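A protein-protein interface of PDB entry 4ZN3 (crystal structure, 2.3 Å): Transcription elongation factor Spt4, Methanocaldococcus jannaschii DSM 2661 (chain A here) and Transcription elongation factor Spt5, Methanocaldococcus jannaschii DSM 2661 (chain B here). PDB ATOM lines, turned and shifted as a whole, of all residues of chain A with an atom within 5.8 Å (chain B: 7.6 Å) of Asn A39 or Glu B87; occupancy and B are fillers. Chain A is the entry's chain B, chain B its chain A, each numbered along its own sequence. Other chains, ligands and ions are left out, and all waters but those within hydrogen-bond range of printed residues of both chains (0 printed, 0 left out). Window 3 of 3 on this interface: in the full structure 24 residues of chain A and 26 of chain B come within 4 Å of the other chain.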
ATOM      1  N   SER A  37      26.831  13.388 -33.187  1.00  0.00           N
ATOM      2  CA  SER A  37      26.713  11.970 -32.918  1.00  0.00           C
ATOM      3  C   SER A  37      25.417  11.456 -33.522  1.00  0.00           C
ATOM      4  O   SER A  37      24.435  12.191 -33.632  1.00  0.00           O
ATOM      5  CB  SER A  37      26.727  11.728 -31.406  1.00  0.00           C
ATOM      6  OG  SER A  37      26.572  10.354 -31.100  1.00  0.00           O
ATOM      7  N   GLU A  38      25.411  10.178 -33.864  1.00  0.00           N
ATOM      8  CA  GLU A  38      24.223   9.521 -34.422  1.00  0.00           C
ATOM      9  C   GLU A  38      23.420   8.857 -33.303  1.00  0.00           C
ATOM     10  O   GLU A  38      22.382   8.242 -33.556  1.00  0.00           O
ATOM     11  CB  GLU A  38      24.591   8.522 -35.541  1.00  0.00           C
ATOM     12  CG  GLU A  38      25.907   7.765 -35.385  1.00  0.00           C
ATOM     13  CD  GLU A  38      26.207   6.867 -36.568  1.00  0.00           C
ATOM     14  OE1 GLU A  38      25.369   5.996 -36.884  1.00  0.00           O
ATOM     15  OE2 GLU A  38      27.286   7.034 -37.179  1.00  0.00           O
ATOM     16  N   ASN A  39      23.885   9.036 -32.065  1.00  0.00           N
ATOM     17  CA  ASN A  39      23.357   8.372 -30.891  1.00  0.00           C
ATOM     18  C   ASN A  39      22.590   9.384 -30.025  1.00  0.00           C
ATOM     19  O   ASN A  39      23.154   9.994 -29.108  1.00  0.00           O
ATOM     20  CB  ASN A  39      24.539   7.757 -30.131  1.00  0.00           C
ATOM     21  CG  ASN A  39      24.140   6.611 -29.231  1.00  0.00           C
ATOM     22  OD1 ASN A  39      23.000   6.522 -28.763  1.00  0.00           O
ATOM     23  ND2 ASN A  39      25.088   5.716 -28.981  1.00  0.00           N
ATOM     24  N   TRP A  40      21.308   9.563 -30.338  1.00  0.00           N
ATOM     25  CA  TRP A  40      20.454  10.538 -29.645  1.00  0.00           C
ATOM     26  C   TRP A  40      18.996  10.099 -29.600  1.00  0.00           C
ATOM     27  O   TRP A  40      18.564   9.270 -30.405  1.00  0.00           O
ATOM     28  CB  TRP A  40      20.561  11.920 -30.314  1.00  0.00           C
ATOM     29  CG  TRP A  40      20.057  11.980 -31.745  1.00  0.00           C
ATOM     30  CD1 TRP A  40      20.792  11.785 -32.878  1.00  0.00           C
ATOM     31  CD2 TRP A  40      18.717  12.262 -32.184  1.00  0.00           C
ATOM     32  NE1 TRP A  40      19.997  11.921 -33.993  1.00  0.00           N
ATOM     33  CE2 TRP A  40      18.719  12.213 -33.597  1.00  0.00           C
ATOM     34  CE3 TRP A  40      17.513  12.548 -31.520  1.00  0.00           C
ATOM     35  CZ2 TRP A  40      17.564  12.440 -34.363  1.00  0.00           C
ATOM     36  CZ3 TRP A  40      16.360  12.777 -32.287  1.00  0.00           C
ATOM     37  CH2 TRP A  40      16.401  12.720 -33.694  1.00  0.00           C
ATOM     38  N   ILE A  41      18.245  10.674 -28.660  1.00  0.00           N
ATOM     39  CA  ILE A  41      16.803  10.413 -28.530  1.00  0.00           C
ATOM     40  C   ILE A  41      16.017  11.668 -28.145  1.00  0.00           C
ATOM     41  O   ILE A  41      16.563  12.624 -27.578  1.00  0.00           O
ATOM     42  CB  ILE A  41      16.475   9.262 -27.531  1.00  0.00           C
ATOM     43  CG1 ILE A  41      17.243   9.403 -26.206  1.00  0.00           C
ATOM     44  CG2 ILE A  41      16.765   7.902 -28.156  1.00  0.00           C
ATOM     45  CD1 ILE A  41      16.587  10.306 -25.187  1.00  0.00           C
ATOM     46  N   SER A  69      18.458  14.179 -25.475  1.00  0.00           N
ATOM     47  CA  SER A  69      19.798  13.778 -25.027  1.00  0.00           C
ATOM     48  C   SER A  69      20.635  13.147 -26.140  1.00  0.00           C
ATOM     49  O   SER A  69      20.104  12.577 -27.096  1.00  0.00           O
ATOM     50  CB  SER A  69      19.712  12.808 -23.850  1.00  0.00           C
ATOM     51  OG  SER A  69      19.279  11.532 -24.279  1.00  0.00           O
ATOM     52  N   VAL A  70      21.951  13.245 -25.967  1.00  0.00           N
ATOM     53  CA  VAL A  70      22.937  12.699 -26.898  1.00  0.00           C
ATOM     54  C   VAL A  70      24.130  12.142 -26.100  1.00  0.00           C
ATOM     55  O   VAL A  70      24.504  12.709 -25.071  1.00  0.00           O
ATOM     56  CB  VAL A  70      23.395  13.789 -27.907  1.00  0.00           C
ATOM     57  CG1 VAL A  70      24.131  14.933 -27.212  1.00  0.00           C
ATOM     58  CG2 VAL A  70      24.247  13.194 -29.024  1.00  0.00           C
ATOM     59  N   LYS A  71      24.710  11.035 -26.571  1.00  0.00           N
ATOM     60  CA  LYS A  71      25.895  10.435 -25.937  1.00  0.00           C
ATOM     61  C   LYS A  71      26.958  10.050 -26.971  1.00  0.00           C
ATOM     62  O   LYS A  71      26.617   9.550 -28.044  1.00  0.00           O
ATOM     63  CB  LYS A  71      25.506   9.211 -25.090  1.00  0.00           C
ATOM     64  CG  LYS A  71      24.849   8.061 -25.847  1.00  0.00           C
ATOM     65  CD  LYS A  71      24.657   6.844 -24.952  1.00  0.00           C
ATOM     66  CE  LYS A  71      24.177   5.646 -25.758  1.00  0.00           C
ATOM     67  NZ  LYS A  71      24.016   4.416 -24.938  1.00  0.00           N
ATOM     68  N   GLU A  72      28.227  10.320 -26.636  1.00  0.00           N
ATOM     69  CA  GLU A  72      29.428   9.844 -27.364  1.00  0.00           C
ATOM     70  C   GLU A  72      30.671  10.584 -26.871  1.00  0.00           C
ATOM     71  O   GLU A  72      31.791  10.268 -27.272  1.00  0.00           O
ATOM     72  CB  GLU A  72      29.319   9.989 -28.900  1.00  0.00           C
ATOM     73  CG  GLU A  72      29.707   8.740 -29.684  1.00  0.00           C
ATOM     74  CD  GLU A  72      28.741   7.573 -29.504  1.00  0.00           C
ATOM     75  OE1 GLU A  72      28.365   7.249 -28.356  1.00  0.00           O
ATOM     76  OE2 GLU A  72      28.366   6.958 -30.527  1.00  0.00           O
ATOM     77  N   LYS B  84      17.447   5.937 -19.392  1.00  0.00           N
ATOM     78  CA  LYS B  84      17.437   4.594 -19.979  1.00  0.00           C
ATOM     79  C   LYS B  84      17.297   4.642 -21.503  1.00  0.00           C
ATOM     80  O   LYS B  84      16.237   4.316 -22.044  1.00  0.00           O
ATOM     81  CB  LYS B  84      16.324   3.739 -19.353  1.00  0.00           C
ATOM     82  N   ILE B  85      18.356   5.089 -22.180  1.00  0.00           N
ATOM     83  CA  ILE B  85      18.409   5.057 -23.654  1.00  0.00           C
ATOM     84  C   ILE B  85      18.482   3.599 -24.166  1.00  0.00           C
ATOM     85  O   ILE B  85      19.563   3.046 -24.393  1.00  0.00           O
ATOM     86  CB  ILE B  85      19.516   5.982 -24.247  1.00  0.00           C
ATOM     87  CG1 ILE B  85      19.468   5.959 -25.782  1.00  0.00           C
ATOM     88  CG2 ILE B  85      20.923   5.642 -23.753  1.00  0.00           C
ATOM     89  CD1 ILE B  85      20.030   7.209 -26.426  1.00  0.00           C
ATOM     90  N   ILE B  86      17.305   2.991 -24.323  1.00  0.00           N
ATOM     91  CA  ILE B  86      17.175   1.589 -24.721  1.00  0.00           C
ATOM     92  C   ILE B  86      17.212   1.495 -26.241  1.00  0.00           C
ATOM     93  O   ILE B  86      16.187   1.661 -26.909  1.00  0.00           O
ATOM     94  CB  ILE B  86      15.870   0.958 -24.162  1.00  0.00           C
ATOM     95  CG1 ILE B  86      15.790   1.114 -22.632  1.00  0.00           C
ATOM     96  CG2 ILE B  86      15.746  -0.511 -24.568  1.00  0.00           C
ATOM     97  CD1 ILE B  86      17.077   0.839 -21.872  1.00  0.00           C
ATOM     98  N   GLU B  87      18.402   1.219 -26.777  1.00  0.00           N
ATOM     99  CA  GLU B  87      18.608   1.119 -28.224  1.00  0.00           C
ATOM    100  C   GLU B  87      17.794  -0.026 -28.830  1.00  0.00           C
ATOM    101  O   GLU B  87      17.482  -1.002 -28.145  1.00  0.00           O
ATOM    102  CB  GLU B  87      20.094   0.937 -28.544  1.00  0.00           C
ATOM    103  CG  GLU B  87      20.947   2.156 -28.222  1.00  0.00           C
ATOM    104  CD  GLU B  87      22.427   1.935 -28.475  1.00  0.00           C
ATOM    105  OE1 GLU B  87      22.914   0.800 -28.299  1.00  0.00           O
ATOM    106  OE2 GLU B  87      23.118   2.904 -28.845  1.00  0.00           O
ATOM    107  N   ASN B  88      17.429   0.124 -30.103  1.00  0.00           N
ATOM    108  CA  ASN B  88      16.706  -0.903 -30.851  1.00  0.00           C
ATOM    109  C   ASN B  88      17.690  -1.682 -31.714  1.00  0.00           C
ATOM    110  O   ASN B  88      18.072  -1.229 -32.800  1.00  0.00           O
ATOM    111  CB  ASN B  88      15.620  -0.272 -31.726  1.00  0.00           C
ATOM    112  CG  ASN B  88      14.808  -1.309 -32.483  1.00  0.00           C
ATOM    113  OD1 ASN B  88      14.340  -2.281 -31.899  1.00  0.00           O
ATOM    114  ND2 ASN B  88      14.630  -1.107 -33.785  1.00  0.00           N
ATOM    115  N   ILE B  89      18.095  -2.855 -31.227  1.00  0.00           N
ATOM    116  CA  ILE B  89      19.103  -3.665 -31.907  1.00  0.00           C
ATOM    117  C   ILE B  89      18.395  -4.505 -32.963  1.00  0.00           C
ATOM    118  O   ILE B  89      17.387  -5.156 -32.683  1.00  0.00           O
ATOM    119  CB  ILE B  89      19.891  -4.602 -30.952  1.00  0.00           C
ATOM    120  CG1 ILE B  89      20.341  -3.890 -29.660  1.00  0.00           C
ATOM    121  CG2 ILE B  89      21.105  -5.181 -31.665  1.00  0.00           C
ATOM    122  CD1 ILE B  89      21.090  -2.592 -29.853  1.00  0.00           C
ATOM    123  N   GLU B  90      18.948  -4.491 -34.171  1.00  0.00           N
ATOM    124  CA  GLU B  90      18.360  -5.170 -35.314  1.00  0.00           C
ATOM    125  C   GLU B  90      19.379  -6.053 -35.990  1.00  0.00           C
ATOM    126  O   GLU B  90      20.583  -5.829 -35.874  1.00  0.00           O
ATOM    127  CB  GLU B  90      17.880  -4.148 -36.336  1.00  0.00           C
ATOM    128  CG  GLU B  90      16.669  -3.344 -35.919  1.00  0.00           C
ATOM    129  CD  GLU B  90      16.376  -2.240 -36.912  1.00  0.00           C
ATOM    130  OE1 GLU B  90      15.534  -2.442 -37.809  1.00  0.00           O
ATOM    131  OE2 GLU B  90      17.026  -1.179 -36.826  1.00  0.00           O
ATOM    132  N   ASP B  93      22.764  -4.821 -37.851  1.00  0.00           N
ATOM    133  CA  ASP B  93      23.495  -3.830 -37.052  1.00  0.00           C
ATOM    134  C   ASP B  93      24.846  -4.382 -36.618  1.00  0.00           C
ATOM    135  O   ASP B  93      24.966  -5.571 -36.310  1.00  0.00           O
ATOM    136  CB  ASP B  93      22.721  -3.426 -35.788  1.00  0.00           C
ATOM    137  CG  ASP B  93      21.459  -2.629 -36.085  1.00  0.00           C
ATOM    138  OD1 ASP B  93      21.235  -2.223 -37.239  1.00  0.00           O
ATOM    139  OD2 ASP B  93      20.678  -2.409 -35.138  1.00  0.00           O
ATOM    140  N   VAL B  95      27.484  -4.190 -33.660  1.00  0.00           N
ATOM    141  CA  VAL B  95      27.473  -3.851 -32.235  1.00  0.00           C
ATOM    142  C   VAL B  95      28.832  -4.078 -31.587  1.00  0.00           C
ATOM    143  O   VAL B  95      29.716  -4.697 -32.175  1.00  0.00           O
ATOM    144  CB  VAL B  95      26.399  -4.636 -31.442  1.00  0.00           C
ATOM    145  CG1 VAL B  95      25.004  -4.287 -31.941  1.00  0.00           C
ATOM    146  CG2 VAL B  95      26.633  -6.147 -31.490  1.00  0.00           C
ATOM    147  N   GLU B  96      28.978  -3.553 -30.374  1.00  0.00           N
ATOM    148  CA  GLU B  96      30.165  -3.764 -29.556  1.00  0.00           C
ATOM    149  C   GLU B  96      29.725  -4.247 -28.180  1.00  0.00           C
ATOM    150  O   GLU B  96      28.773  -3.709 -27.603  1.00  0.00           O
ATOM    151  CB  GLU B  96      30.966  -2.468 -29.439  1.00  0.00           C
ATOM    152  CG  GLU B  96      32.259  -2.591 -28.647  1.00  0.00           C
ATOM    153  CD  GLU B  96      33.071  -1.313 -28.676  1.00  0.00           C
ATOM    154  OE1 GLU B  96      33.090  -0.597 -27.654  1.00  0.00           O
ATOM    155  OE2 GLU B  96      33.679  -1.018 -29.727  1.00  0.00           O
ATOM    156  N   ILE B  98      29.728  -4.543 -24.352  1.00  0.00           N
ATOM    157  CA  ILE B  98      29.978  -3.464 -23.396  1.00  0.00           C
ATOM    158  C   ILE B  98      30.924  -3.881 -22.271  1.00  0.00           C
ATOM    159  O   ILE B  98      31.873  -3.161 -21.971  1.00  0.00           O
ATOM    160  CB  ILE B  98      28.663  -2.933 -22.774  1.00  0.00           C
ATOM    161  CG1 ILE B  98      27.747  -2.365 -23.867  1.00  0.00           C
ATOM    162  CG2 ILE B  98      28.960  -1.844 -21.739  1.00  0.00           C
ATOM    163  CD1 ILE B  98      26.308  -2.173 -23.440  1.00  0.00           C
ATOM    164  N   LYS B 114      13.228 -11.398 -29.527  1.00  0.00           N
ATOM    165  CA  LYS B 114      12.401 -10.463 -28.763  1.00  0.00           C
ATOM    166  C   LYS B 114      11.819 -11.120 -27.519  1.00  0.00           C
ATOM    167  O   LYS B 114      11.839 -10.523 -26.441  1.00  0.00           O
ATOM    168  CB  LYS B 114      11.277  -9.902 -29.638  1.00  0.00           C
ATOM    169  CG  LYS B 114      11.759  -9.062 -30.812  1.00  0.00           C
ATOM    170  CD  LYS B 114      12.554  -7.853 -30.336  1.00  0.00           C
ATOM    171  CE  LYS B 114      12.646  -6.768 -31.390  1.00  0.00           C
ATOM    172  NZ  LYS B 114      13.190  -5.517 -30.797  1.00  0.00           N
ATOM    173  N   VAL B 136      20.523  -8.290 -24.950  1.00  0.00           N
ATOM    174  CA  VAL B 136      20.599  -6.993 -25.657  1.00  0.00           C
ATOM    175  C   VAL B 136      21.389  -5.942 -24.874  1.00  0.00           C
ATOM    176  O   VAL B 136      22.234  -5.248 -25.439  1.00  0.00           O
ATOM    177  CB  VAL B 136      19.206  -6.409 -26.030  1.00  0.00           C
ATOM    178  CG1 VAL B 136      18.548  -7.234 -27.125  1.00  0.00           C
ATOM    179  CG2 VAL B 136      18.281  -6.270 -24.820  1.00  0.00           C
ATOM    180  N   VAL B 139      25.316  -5.010 -24.957  1.00  0.00           N
ATOM    181  CA  VAL B 139      25.761  -4.636 -26.293  1.00  0.00           C
ATOM    182  C   VAL B 139      25.302  -3.208 -26.610  1.00  0.00           C
ATOM    183  O   VAL B 139      24.237  -2.784 -26.159  1.00  0.00           O
ATOM    184  CB  VAL B 139      25.223  -5.683 -27.310  1.00  0.00           C
ATOM    185  CG1 VAL B 139      24.509  -5.065 -28.510  1.00  0.00           C
ATOM    186  CG2 VAL B 139      26.338  -6.630 -27.736  1.00  0.00           C
ATOM    187  N   LYS B 140      26.111  -2.478 -27.377  1.00  0.00           N
ATOM    188  CA  LYS B 140      25.726  -1.158 -27.880  1.00  0.00           C
ATOM    189  C   LYS B 140      25.912  -1.092 -29.393  1.00  0.00           C
ATOM    190  O   LYS B 140      26.793  -1.757 -29.942  1.00  0.00           O
ATOM    191  CB  LYS B 140      26.524  -0.042 -27.192  1.00  0.00           C
ATOM    192  CG  LYS B 140      28.032  -0.127 -27.361  1.00  0.00           C
ATOM    193  CD  LYS B 140      28.715   1.145 -26.883  1.00  0.00           C
ATOM    194  CE  LYS B 140      30.210   1.081 -27.142  1.00  0.00           C
ATOM    195  NZ  LYS B 140      30.902   2.337 -26.741  1.00  0.00           N
ATOM    196  N   ILE B 141      25.093  -0.269 -30.049  1.00  0.00           N
ATOM    197  CA  ILE B 141      25.139  -0.106 -31.503  1.00  0.00           C
ATOM    198  C   ILE B 141      26.394   0.678 -31.872  1.00  0.00           C
ATOM    199  O   ILE B 141      26.658   1.726 -31.298  1.00  0.00           O
ATOM    200  CB  ILE B 141      23.868   0.603 -32.057  1.00  0.00           C
ATOM    201  CG1 ILE B 141      22.626  -0.256 -31.784  1.00  0.00           C
ATOM    202  CG2 ILE B 141      23.990   0.862 -33.559  1.00  0.00           C
ATOM    203  CD1 ILE B 141      21.297   0.405 -32.089  1.00  0.00           C
ATOM    204  N   VAL B 142      27.170   0.131 -32.803  1.00  0.00           N
ATOM    205  CA  VAL B 142      28.300   0.821 -33.430  1.00  0.00           C
ATOM    206  C   VAL B 142      27.848   1.444 -34.747  1.00  0.00           C
ATOM    207  O   VAL B 142      28.215   2.574 -35.065  1.00  0.00           O
ATOM    208  CB  VAL B 142      29.471  -0.152 -33.705  1.00  0.00           C
ATOM    209  CG1 VAL B 142      30.566   0.502 -34.541  1.00  0.00           C
ATOM    210  CG2 VAL B 142      30.046  -0.665 -32.392  1.00  0.00           C
ATOM    211  N   LYS B 144      24.370   1.140 -37.751  1.00  0.00           N
ATOM    212  CA  LYS B 144      23.058   0.592 -38.087  1.00  0.00           C
ATOM    213  C   LYS B 144      23.115  -0.189 -39.389  1.00  0.00           C
ATOM    214  O   LYS B 144      23.922   0.106 -40.262  1.00  0.00           O
ATOM    215  CB  LYS B 144      22.009   1.706 -38.189  1.00  0.00           C
ATOM    216  CG  LYS B 144      21.630   2.351 -36.855  1.00  0.00           C
ATOM    217  CD  LYS B 144      20.991   1.384 -35.858  1.00  0.00           C
ATOM    218  CE  LYS B 144      19.717   0.737 -36.389  1.00  0.00           C
ATOM    219  NZ  LYS B 144      19.034  -0.079 -35.352  1.00  0.00           N
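OE2 of Glu B87 is in hydrogen-bond range of ND2 of Asn A39, 3.4 Å away.
The backbone NH (N) of Ile B141 is in hydrogen-bond range of the side-chain carboxylate (OE1) of Glu B87 (3.0 Å). OG of Ser A37 sits at hydrogen-bond distance from N of Asn A39. The backbone carbonyl oxygen of Lys A71 sits at hydrogen-bond distance from the side-chain hydroxyl of Ser A37. N of Lys A71 sits at hydrogen-bond distance from O of Asn A39 (3.2 Å). O of Ser A69 sits at hydrogen-bond distance from N of Ile A41 (3.1 Å).
Ile B85 touches Asn A39 (CD1 to OD1, 3.8 Å). Ile A41 touches Ile B85 (CG1 to CD1, 3.6 Å). Lys A71 touches Ile B85 (NZ to CG2, 3.5 Å).
Of chain B, only Ile B85 (3.8 Å) and Glu B87 (3.4 Å) come within 4 Å of Asn A39. Of the printed residues of chain A, Glu B87 touches Asn A39. Printed residues of chain B within 4 Å of Lys A71: Ile B85 (3.5 Å). Of the printed residues of chain A, Ile B85 touches Asn A39 (3.8 Å), Ile A41 (3.6 Å) and Lys A71 (3.5 Å). Printed residues of chain B within 4 Å of Ile A41: Ile B85 (3.6 Å). Glu A38 touches none of the printed residues of chain B. Glu B96 touches none of the printed residues of chain A. The nearest printed residue of chain B that does not touch Lys A71 is Glu B87 (4.3 Å).
Of the 9 printed residues of chain A, 3 touch a printed residue of chain B. Printed residues of chain A that touch a printed residue of chain B: Asn A39, Ile A41 and Lys A71. Hydrophobic or aromatic side chains of chain A within 4 Å of the printed part of chain B: Ile A41. Of the 18 printed residues of chain B, 2 touch a printed residue of chain A. Printed residues of chain B that touch a printed residue of chain A: Ile B85 and Glu B87. Hydrophobic or aromatic side chains of chain B that line the printed part of chain A: Ile B85. Among the printed residues, 4 pairs touch across the chains.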
